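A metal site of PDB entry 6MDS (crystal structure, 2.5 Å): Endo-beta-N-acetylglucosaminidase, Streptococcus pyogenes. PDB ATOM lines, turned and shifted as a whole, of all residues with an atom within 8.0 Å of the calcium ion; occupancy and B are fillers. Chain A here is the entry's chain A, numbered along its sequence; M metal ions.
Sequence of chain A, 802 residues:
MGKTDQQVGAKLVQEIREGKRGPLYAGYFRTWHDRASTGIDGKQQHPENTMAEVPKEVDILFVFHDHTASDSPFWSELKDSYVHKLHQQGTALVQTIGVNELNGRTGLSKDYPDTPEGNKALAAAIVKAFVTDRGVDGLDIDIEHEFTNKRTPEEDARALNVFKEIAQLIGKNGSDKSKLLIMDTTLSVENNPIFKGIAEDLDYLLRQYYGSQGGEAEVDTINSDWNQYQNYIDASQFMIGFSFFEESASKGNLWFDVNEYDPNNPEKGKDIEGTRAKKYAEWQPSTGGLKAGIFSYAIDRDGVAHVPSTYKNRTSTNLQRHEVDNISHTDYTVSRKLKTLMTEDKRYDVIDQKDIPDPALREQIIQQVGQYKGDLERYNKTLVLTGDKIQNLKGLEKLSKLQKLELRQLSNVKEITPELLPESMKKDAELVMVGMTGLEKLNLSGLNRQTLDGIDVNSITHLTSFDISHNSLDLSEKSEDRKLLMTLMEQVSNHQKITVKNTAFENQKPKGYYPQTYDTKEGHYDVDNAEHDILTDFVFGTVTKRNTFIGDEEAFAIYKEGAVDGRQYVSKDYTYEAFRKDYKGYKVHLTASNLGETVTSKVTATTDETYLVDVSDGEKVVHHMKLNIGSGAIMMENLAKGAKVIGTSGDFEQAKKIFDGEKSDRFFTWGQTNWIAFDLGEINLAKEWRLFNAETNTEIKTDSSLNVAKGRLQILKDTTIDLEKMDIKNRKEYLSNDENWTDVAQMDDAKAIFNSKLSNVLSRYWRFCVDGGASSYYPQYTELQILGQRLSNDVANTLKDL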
ATOM      1  N   GLN A 654      30.200  -2.830 -28.456  1.00  0.00           N
ATOM      2  CA  GLN A 654      28.808  -2.624 -28.075  1.00  0.00           C
ATOM      3  C   GLN A 654      27.871  -3.104 -29.174  1.00  0.00           C
ATOM      4  O   GLN A 654      26.747  -3.510 -28.879  1.00  0.00           O
ATOM      5  CB  GLN A 654      28.536  -1.152 -27.774  1.00  0.00           C
ATOM      6  CG  GLN A 654      29.362  -0.571 -26.665  1.00  0.00           C
ATOM      7  CD  GLN A 654      28.929  -1.092 -25.330  1.00  0.00           C
ATOM      8  OE1 GLN A 654      27.730  -1.183 -25.032  1.00  0.00           O
ATOM      9  NE2 GLN A 654      29.901  -1.455 -24.496  1.00  0.00           N
ATOM     10  N   ALA A 655      28.327  -3.092 -30.438  1.00  0.00           N
ATOM     11  CA  ALA A 655      27.457  -3.486 -31.536  1.00  0.00           C
ATOM     12  C   ALA A 655      27.179  -4.981 -31.494  1.00  0.00           C
ATOM     13  O   ALA A 655      26.046  -5.426 -31.721  1.00  0.00           O
ATOM     14  CB  ALA A 655      28.109  -3.108 -32.869  1.00  0.00           C
ATOM     15  N   LYS A 656      28.197  -5.763 -31.146  1.00  0.00           N
ATOM     16  CA  LYS A 656      28.078  -7.201 -31.088  1.00  0.00           C
ATOM     17  C   LYS A 656      27.047  -7.669 -30.060  1.00  0.00           C
ATOM     18  O   LYS A 656      26.548  -8.784 -30.197  1.00  0.00           O
ATOM     19  CB  LYS A 656      29.503  -7.765 -30.968  1.00  0.00           C
ATOM     20  CG  LYS A 656      30.290  -8.094 -32.259  1.00  0.00           C
ATOM     21  CD  LYS A 656      31.748  -8.400 -31.782  1.00  0.00           C
ATOM     22  CE  LYS A 656      33.003  -7.920 -32.557  1.00  0.00           C
ATOM     23  NZ  LYS A 656      33.450  -9.251 -33.295  1.00  0.00           N
ATOM     24  N   LYS A 657      26.631  -6.805 -29.126  1.00  0.00           N
ATOM     25  CA  LYS A 657      25.660  -7.224 -28.121  1.00  0.00           C
ATOM     26  C   LYS A 657      24.207  -7.128 -28.598  1.00  0.00           C
ATOM     27  O   LYS A 657      23.326  -7.621 -27.884  1.00  0.00           O
ATOM     28  CB  LYS A 657      25.863  -6.409 -26.834  1.00  0.00           C
ATOM     29  CG  LYS A 657      27.273  -6.610 -26.251  1.00  0.00           C
ATOM     30  CD  LYS A 657      27.298  -6.689 -24.729  1.00  0.00           C
ATOM     31  CE  LYS A 657      28.735  -6.750 -24.187  1.00  0.00           C
ATOM     32  NZ  LYS A 657      29.260  -5.361 -23.989  1.00  0.00           N
ATOM     33  N   ILE A 658      23.913  -6.527 -29.749  1.00  0.00           N
ATOM     34  CA  ILE A 658      22.516  -6.554 -30.232  1.00  0.00           C
ATOM     35  C   ILE A 658      22.135  -7.893 -30.859  1.00  0.00           C
ATOM     36  O   ILE A 658      20.981  -8.074 -31.276  1.00  0.00           O
ATOM     37  CB  ILE A 658      22.211  -5.398 -31.193  1.00  0.00           C
ATOM     38  CG1 ILE A 658      22.974  -5.572 -32.509  1.00  0.00           C
ATOM     39  CG2 ILE A 658      22.458  -4.041 -30.528  1.00  0.00           C
ATOM     40  CD1 ILE A 658      22.367  -4.802 -33.656  1.00  0.00           C
ATOM     41  N   PHE A 659      23.066  -8.826 -30.956  1.00  0.00           N
ATOM     42  CA  PHE A 659      22.814 -10.134 -31.545  1.00  0.00           C
ATOM     43  C   PHE A 659      23.093 -11.263 -30.553  1.00  0.00           C
ATOM     44  O   PHE A 659      23.216 -12.419 -30.961  1.00  0.00           O
ATOM     45  CB  PHE A 659      23.630 -10.328 -32.819  1.00  0.00           C
ATOM     46  CG  PHE A 659      23.364  -9.288 -33.883  1.00  0.00           C
ATOM     47  CD1 PHE A 659      22.109  -9.196 -34.477  1.00  0.00           C
ATOM     48  CD2 PHE A 659      24.366  -8.415 -34.284  1.00  0.00           C
ATOM     49  CE1 PHE A 659      21.864  -8.254 -35.470  1.00  0.00           C
ATOM     50  CE2 PHE A 659      24.122  -7.472 -35.278  1.00  0.00           C
ATOM     51  CZ  PHE A 659      22.867  -7.397 -35.869  1.00  0.00           C
ATOM     52  N   ASP A 660      23.198 -10.974 -29.258  1.00  0.00           N
ATOM     53  CA  ASP A 660      23.202 -12.060 -28.299  1.00  0.00           C
ATOM     54  C   ASP A 660      21.757 -12.484 -28.051  1.00  0.00           C
ATOM     55  O   ASP A 660      20.920 -12.398 -28.953  1.00  0.00           O
ATOM     56  CB  ASP A 660      23.951 -11.690 -27.002  1.00  0.00           C
ATOM     57  CG  ASP A 660      23.437 -10.401 -26.348  1.00  0.00           C
ATOM     58  OD1 ASP A 660      22.253 -10.054 -26.562  1.00  0.00           O
ATOM     59  OD2 ASP A 660      24.206  -9.747 -25.590  1.00  0.00           O
ATOM     60  N   GLY A 661      21.441 -12.978 -26.878  1.00  0.00           N
ATOM     61  CA  GLY A 661      20.056 -13.390 -26.736  1.00  0.00           C
ATOM     62  C   GLY A 661      19.287 -12.435 -25.869  1.00  0.00           C
ATOM     63  O   GLY A 661      18.081 -12.604 -25.656  1.00  0.00           O
ATOM     64  N   GLU A 662      19.965 -11.416 -25.365  1.00  0.00           N
ATOM     65  CA  GLU A 662      19.541 -10.698 -24.168  1.00  0.00           C
ATOM     66  C   GLU A 662      19.074  -9.296 -24.496  1.00  0.00           C
ATOM     67  O   GLU A 662      19.183  -8.816 -25.615  1.00  0.00           O
ATOM     68  CB  GLU A 662      20.687 -10.644 -23.151  1.00  0.00           C
ATOM     69  CG  GLU A 662      21.504 -11.913 -23.097  1.00  0.00           C
ATOM     70  CD  GLU A 662      20.725 -13.118 -22.609  1.00  0.00           C
ATOM     71  OE1 GLU A 662      19.582 -12.950 -22.103  1.00  0.00           O
ATOM     72  OE2 GLU A 662      21.250 -14.247 -22.754  1.00  0.00           O
ATOM     73  N   LYS A 663      18.528  -8.648 -23.479  1.00  0.00           N
ATOM     74  CA  LYS A 663      18.159  -7.236 -23.538  1.00  0.00           C
ATOM     75  C   LYS A 663      18.871  -6.456 -22.436  1.00  0.00           C
ATOM     76  O   LYS A 663      18.432  -5.362 -22.064  1.00  0.00           O
ATOM     77  CB  LYS A 663      16.635  -7.078 -23.459  1.00  0.00           C
ATOM     78  CG  LYS A 663      15.855  -8.016 -24.423  1.00  0.00           C
ATOM     79  CD  LYS A 663      14.341  -7.886 -24.286  1.00  0.00           C
ATOM     80  CE  LYS A 663      13.799  -8.558 -23.015  1.00  0.00           C
ATOM     81  NZ  LYS A 663      12.976  -7.620 -22.166  1.00  0.00           N
ATOM     82  N   SER A 664      19.977  -6.996 -21.927  1.00  0.00           N
ATOM     83  CA  SER A 664      20.713  -6.455 -20.775  1.00  0.00           C
ATOM     84  C   SER A 664      21.877  -5.564 -21.208  1.00  0.00           C
ATOM     85  O   SER A 664      22.919  -5.512 -20.554  1.00  0.00           O
ATOM     86  CB  SER A 664      21.207  -7.600 -19.901  1.00  0.00           C
ATOM     87  OG  SER A 664      22.116  -8.409 -20.621  1.00  0.00           O
ATOM     88  N   ASP A 665      21.686  -4.806 -22.279  1.00  0.00           N
ATOM     89  CA  ASP A 665      22.745  -4.054 -22.938  1.00  0.00           C
ATOM     90  C   ASP A 665      22.060  -2.982 -23.776  1.00  0.00           C
ATOM     91  O   ASP A 665      20.850  -3.017 -23.981  1.00  0.00           O
ATOM     92  CB  ASP A 665      23.630  -4.959 -23.795  1.00  0.00           C
ATOM     93  CG  ASP A 665      22.822  -5.739 -24.857  1.00  0.00           C
ATOM     94  OD1 ASP A 665      22.463  -5.124 -25.889  1.00  0.00           O
ATOM     95  OD2 ASP A 665      22.567  -6.958 -24.682  1.00  0.00           O
ATOM     96  N   ARG A 666      22.843  -2.038 -24.259  1.00  0.00           N
ATOM     97  CA  ARG A 666      22.245  -0.975 -25.048  1.00  0.00           C
ATOM     98  C   ARG A 666      23.276  -0.493 -26.056  1.00  0.00           C
ATOM     99  O   ARG A 666      24.469  -0.445 -25.741  1.00  0.00           O
ATOM    100  CB  ARG A 666      21.767   0.160 -24.145  1.00  0.00           C
ATOM    101  CG  ARG A 666      22.866   0.663 -23.231  1.00  0.00           C
ATOM    102  CD  ARG A 666      22.435   1.836 -22.399  1.00  0.00           C
ATOM    103  NE  ARG A 666      23.563   2.401 -21.656  1.00  0.00           N
ATOM    104  CZ  ARG A 666      23.437   3.161 -20.563  1.00  0.00           C
ATOM    105  NH1 ARG A 666      22.229   3.431 -20.092  1.00  0.00           N
ATOM    106  NH2 ARG A 666      24.520   3.653 -19.962  1.00  0.00           N
ATOM    107  N   PHE A 667      22.817  -0.167 -27.256  1.00  0.00           N
ATOM    108  CA  PHE A 667      23.675   0.359 -28.309  1.00  0.00           C
ATOM    109  C   PHE A 667      23.232   1.764 -28.664  1.00  0.00           C
ATOM    110  O   PHE A 667      22.085   1.972 -29.080  1.00  0.00           O
ATOM    111  CB  PHE A 667      23.672  -0.514 -29.562  1.00  0.00           C
ATOM    112  CG  PHE A 667      24.489   0.048 -30.669  1.00  0.00           C
ATOM    113  CD1 PHE A 667      23.913   0.897 -31.613  1.00  0.00           C
ATOM    114  CD2 PHE A 667      25.848  -0.211 -30.743  1.00  0.00           C
ATOM    115  CE1 PHE A 667      24.680   1.458 -32.581  1.00  0.00           C
ATOM    116  CE2 PHE A 667      26.626   0.352 -31.742  1.00  0.00           C
ATOM    117  CZ  PHE A 667      26.045   1.188 -32.647  1.00  0.00           C
ATOM    118  N   PHE A 692      14.071  -4.632 -30.376  1.00  0.00           N
ATOM    119  CA  PHE A 692      13.766  -4.365 -28.981  1.00  0.00           C
ATOM    120  C   PHE A 692      14.329  -2.997 -28.636  1.00  0.00           C
ATOM    121  O   PHE A 692      15.544  -2.783 -28.711  1.00  0.00           O
ATOM    122  CB  PHE A 692      14.332  -5.483 -28.101  1.00  0.00           C
ATOM    123  CG  PHE A 692      13.659  -6.800 -28.307  1.00  0.00           C
ATOM    124  CD1 PHE A 692      13.916  -7.565 -29.432  1.00  0.00           C
ATOM    125  CD2 PHE A 692      12.736  -7.279 -27.370  1.00  0.00           C
ATOM    126  CE1 PHE A 692      13.279  -8.788 -29.619  1.00  0.00           C
ATOM    127  CE2 PHE A 692      12.078  -8.496 -27.561  1.00  0.00           C
ATOM    128  CZ  PHE A 692      12.361  -9.261 -28.676  1.00  0.00           C
ATOM    129  N   THR A 696      13.262  -1.723 -23.329  1.00  0.00           N
ATOM    130  CA  THR A 696      13.306  -3.137 -22.972  1.00  0.00           C
ATOM    131  C   THR A 696      14.573  -3.518 -22.206  1.00  0.00           C
ATOM    132  O   THR A 696      14.755  -4.696 -21.892  1.00  0.00           O
ATOM    133  CB  THR A 696      13.185  -4.014 -24.231  1.00  0.00           C
ATOM    134  OG1 THR A 696      14.396  -3.978 -24.981  1.00  0.00           O
ATOM    135  CG2 THR A 696      12.049  -3.530 -25.098  1.00  0.00           C
ATOM    136  N   TYR A 781      18.873   1.007 -28.389  1.00  0.00           N
ATOM    137  CA  TYR A 781      18.094  -0.212 -28.514  1.00  0.00           C
ATOM    138  C   TYR A 781      18.954  -1.380 -28.060  1.00  0.00           C
ATOM    139  O   TYR A 781      20.193  -1.300 -28.023  1.00  0.00           O
ATOM    140  CB  TYR A 781      17.545  -0.420 -29.938  1.00  0.00           C
ATOM    141  CG  TYR A 781      18.564  -0.654 -31.021  1.00  0.00           C
ATOM    142  CD1 TYR A 781      19.177   0.424 -31.689  1.00  0.00           C
ATOM    143  CD2 TYR A 781      18.906  -1.939 -31.405  1.00  0.00           C
ATOM    144  CE1 TYR A 781      20.113   0.217 -32.687  1.00  0.00           C
ATOM    145  CE2 TYR A 781      19.821  -2.171 -32.425  1.00  0.00           C
ATOM    146  CZ  TYR A 781      20.431  -1.084 -33.065  1.00  0.00           C
ATOM    147  OH  TYR A 781      21.358  -1.336 -34.056  1.00  0.00           O
ATOM    148  N   THR A 782      18.288  -2.486 -27.704  1.00  0.00           N
ATOM    149  CA  THR A 782      18.969  -3.574 -27.022  1.00  0.00           C
ATOM    150  C   THR A 782      19.188  -4.805 -27.888  1.00  0.00           C
ATOM    151  O   THR A 782      20.182  -5.498 -27.689  1.00  0.00           O
ATOM    152  CB  THR A 782      18.188  -3.993 -25.770  1.00  0.00           C
ATOM    153  OG1 THR A 782      16.931  -4.543 -26.173  1.00  0.00           O
ATOM    154  CG2 THR A 782      17.935  -2.811 -24.871  1.00  0.00           C
ATOM    155  N   GLU A 783      18.321  -5.079 -28.855  1.00  0.00           N
ATOM    156  CA  GLU A 783      18.472  -6.338 -29.568  1.00  0.00           C
ATOM    157  C   GLU A 783      17.734  -6.295 -30.896  1.00  0.00           C
ATOM    158  O   GLU A 783      16.756  -5.568 -31.058  1.00  0.00           O
ATOM    159  CB  GLU A 783      18.005  -7.491 -28.652  1.00  0.00           C
ATOM    160  CG  GLU A 783      17.748  -8.812 -29.311  1.00  0.00           C
ATOM    161  CD  GLU A 783      19.034  -9.602 -29.359  1.00  0.00           C
ATOM    162  OE1 GLU A 783      19.989  -9.313 -28.619  1.00  0.00           O
ATOM    163  OE2 GLU A 783      19.097 -10.532 -30.162  1.00  0.00           O
ATOM    164  N   LEU A 784      18.245  -7.046 -31.852  1.00  0.00           N
ATOM    165  CA  LEU A 784      17.648  -7.082 -33.191  1.00  0.00           C
ATOM    166  C   LEU A 784      17.542  -8.527 -33.677  1.00  0.00           C
ATOM    167  O   LEU A 784      18.440  -9.349 -33.454  1.00  0.00           O
ATOM    168  CB  LEU A 784      18.426  -6.191 -34.166  1.00  0.00           C
ATOM    169  CG  LEU A 784      17.787  -6.027 -35.547  1.00  0.00           C
ATOM    170  CD1 LEU A 784      16.559  -5.142 -35.520  1.00  0.00           C
ATOM    171  CD2 LEU A 784      18.814  -5.355 -36.408  1.00  0.00           C
HETATM  172 CA    CA M   1      21.254  -7.507 -26.810  1.00  0.00          CA
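The backbone NH (N) of Phe 692 is in hydrogen-bond range of the backbone carbonyl oxygen (O) of Glu 783. The backbone NH of Thr 782 is in hydrogen-bond range of the backbone carbonyl oxygen of Phe 692 (2.9 Å). The backbone carbonyl oxygen of Ile 658 lies within hydrogen-bond range of the backbone NH of Leu 784 (3.0 Å). The side-chain hydroxyl of Thr 782 is in hydrogen-bond range of the side-chain hydroxyl of Thr 696 (2.9 Å).
Residues that only touch the calcium ion: Ile 658 (3.8 Å). Along chain A the residues within 4 Å of the calcium ion span positions 657 to 783. The nearest printed residue that does not touch the calcium ion is Lys 663 (4.5 Å).
The calcium ion is bound by O of Lys 657 (2.3 Å), O of Thr 782 (2.4 Å), OD2 of Asp 665 (2.6 Å), O of Glu 662 (2.7 Å), OD1 of Asp 660 (2.7 Å), OD1 of Asp 665 (2.8 Å) and OE1 of Glu 783 (2.9 Å). The calcium ion has seven donor atoms within binding distance.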
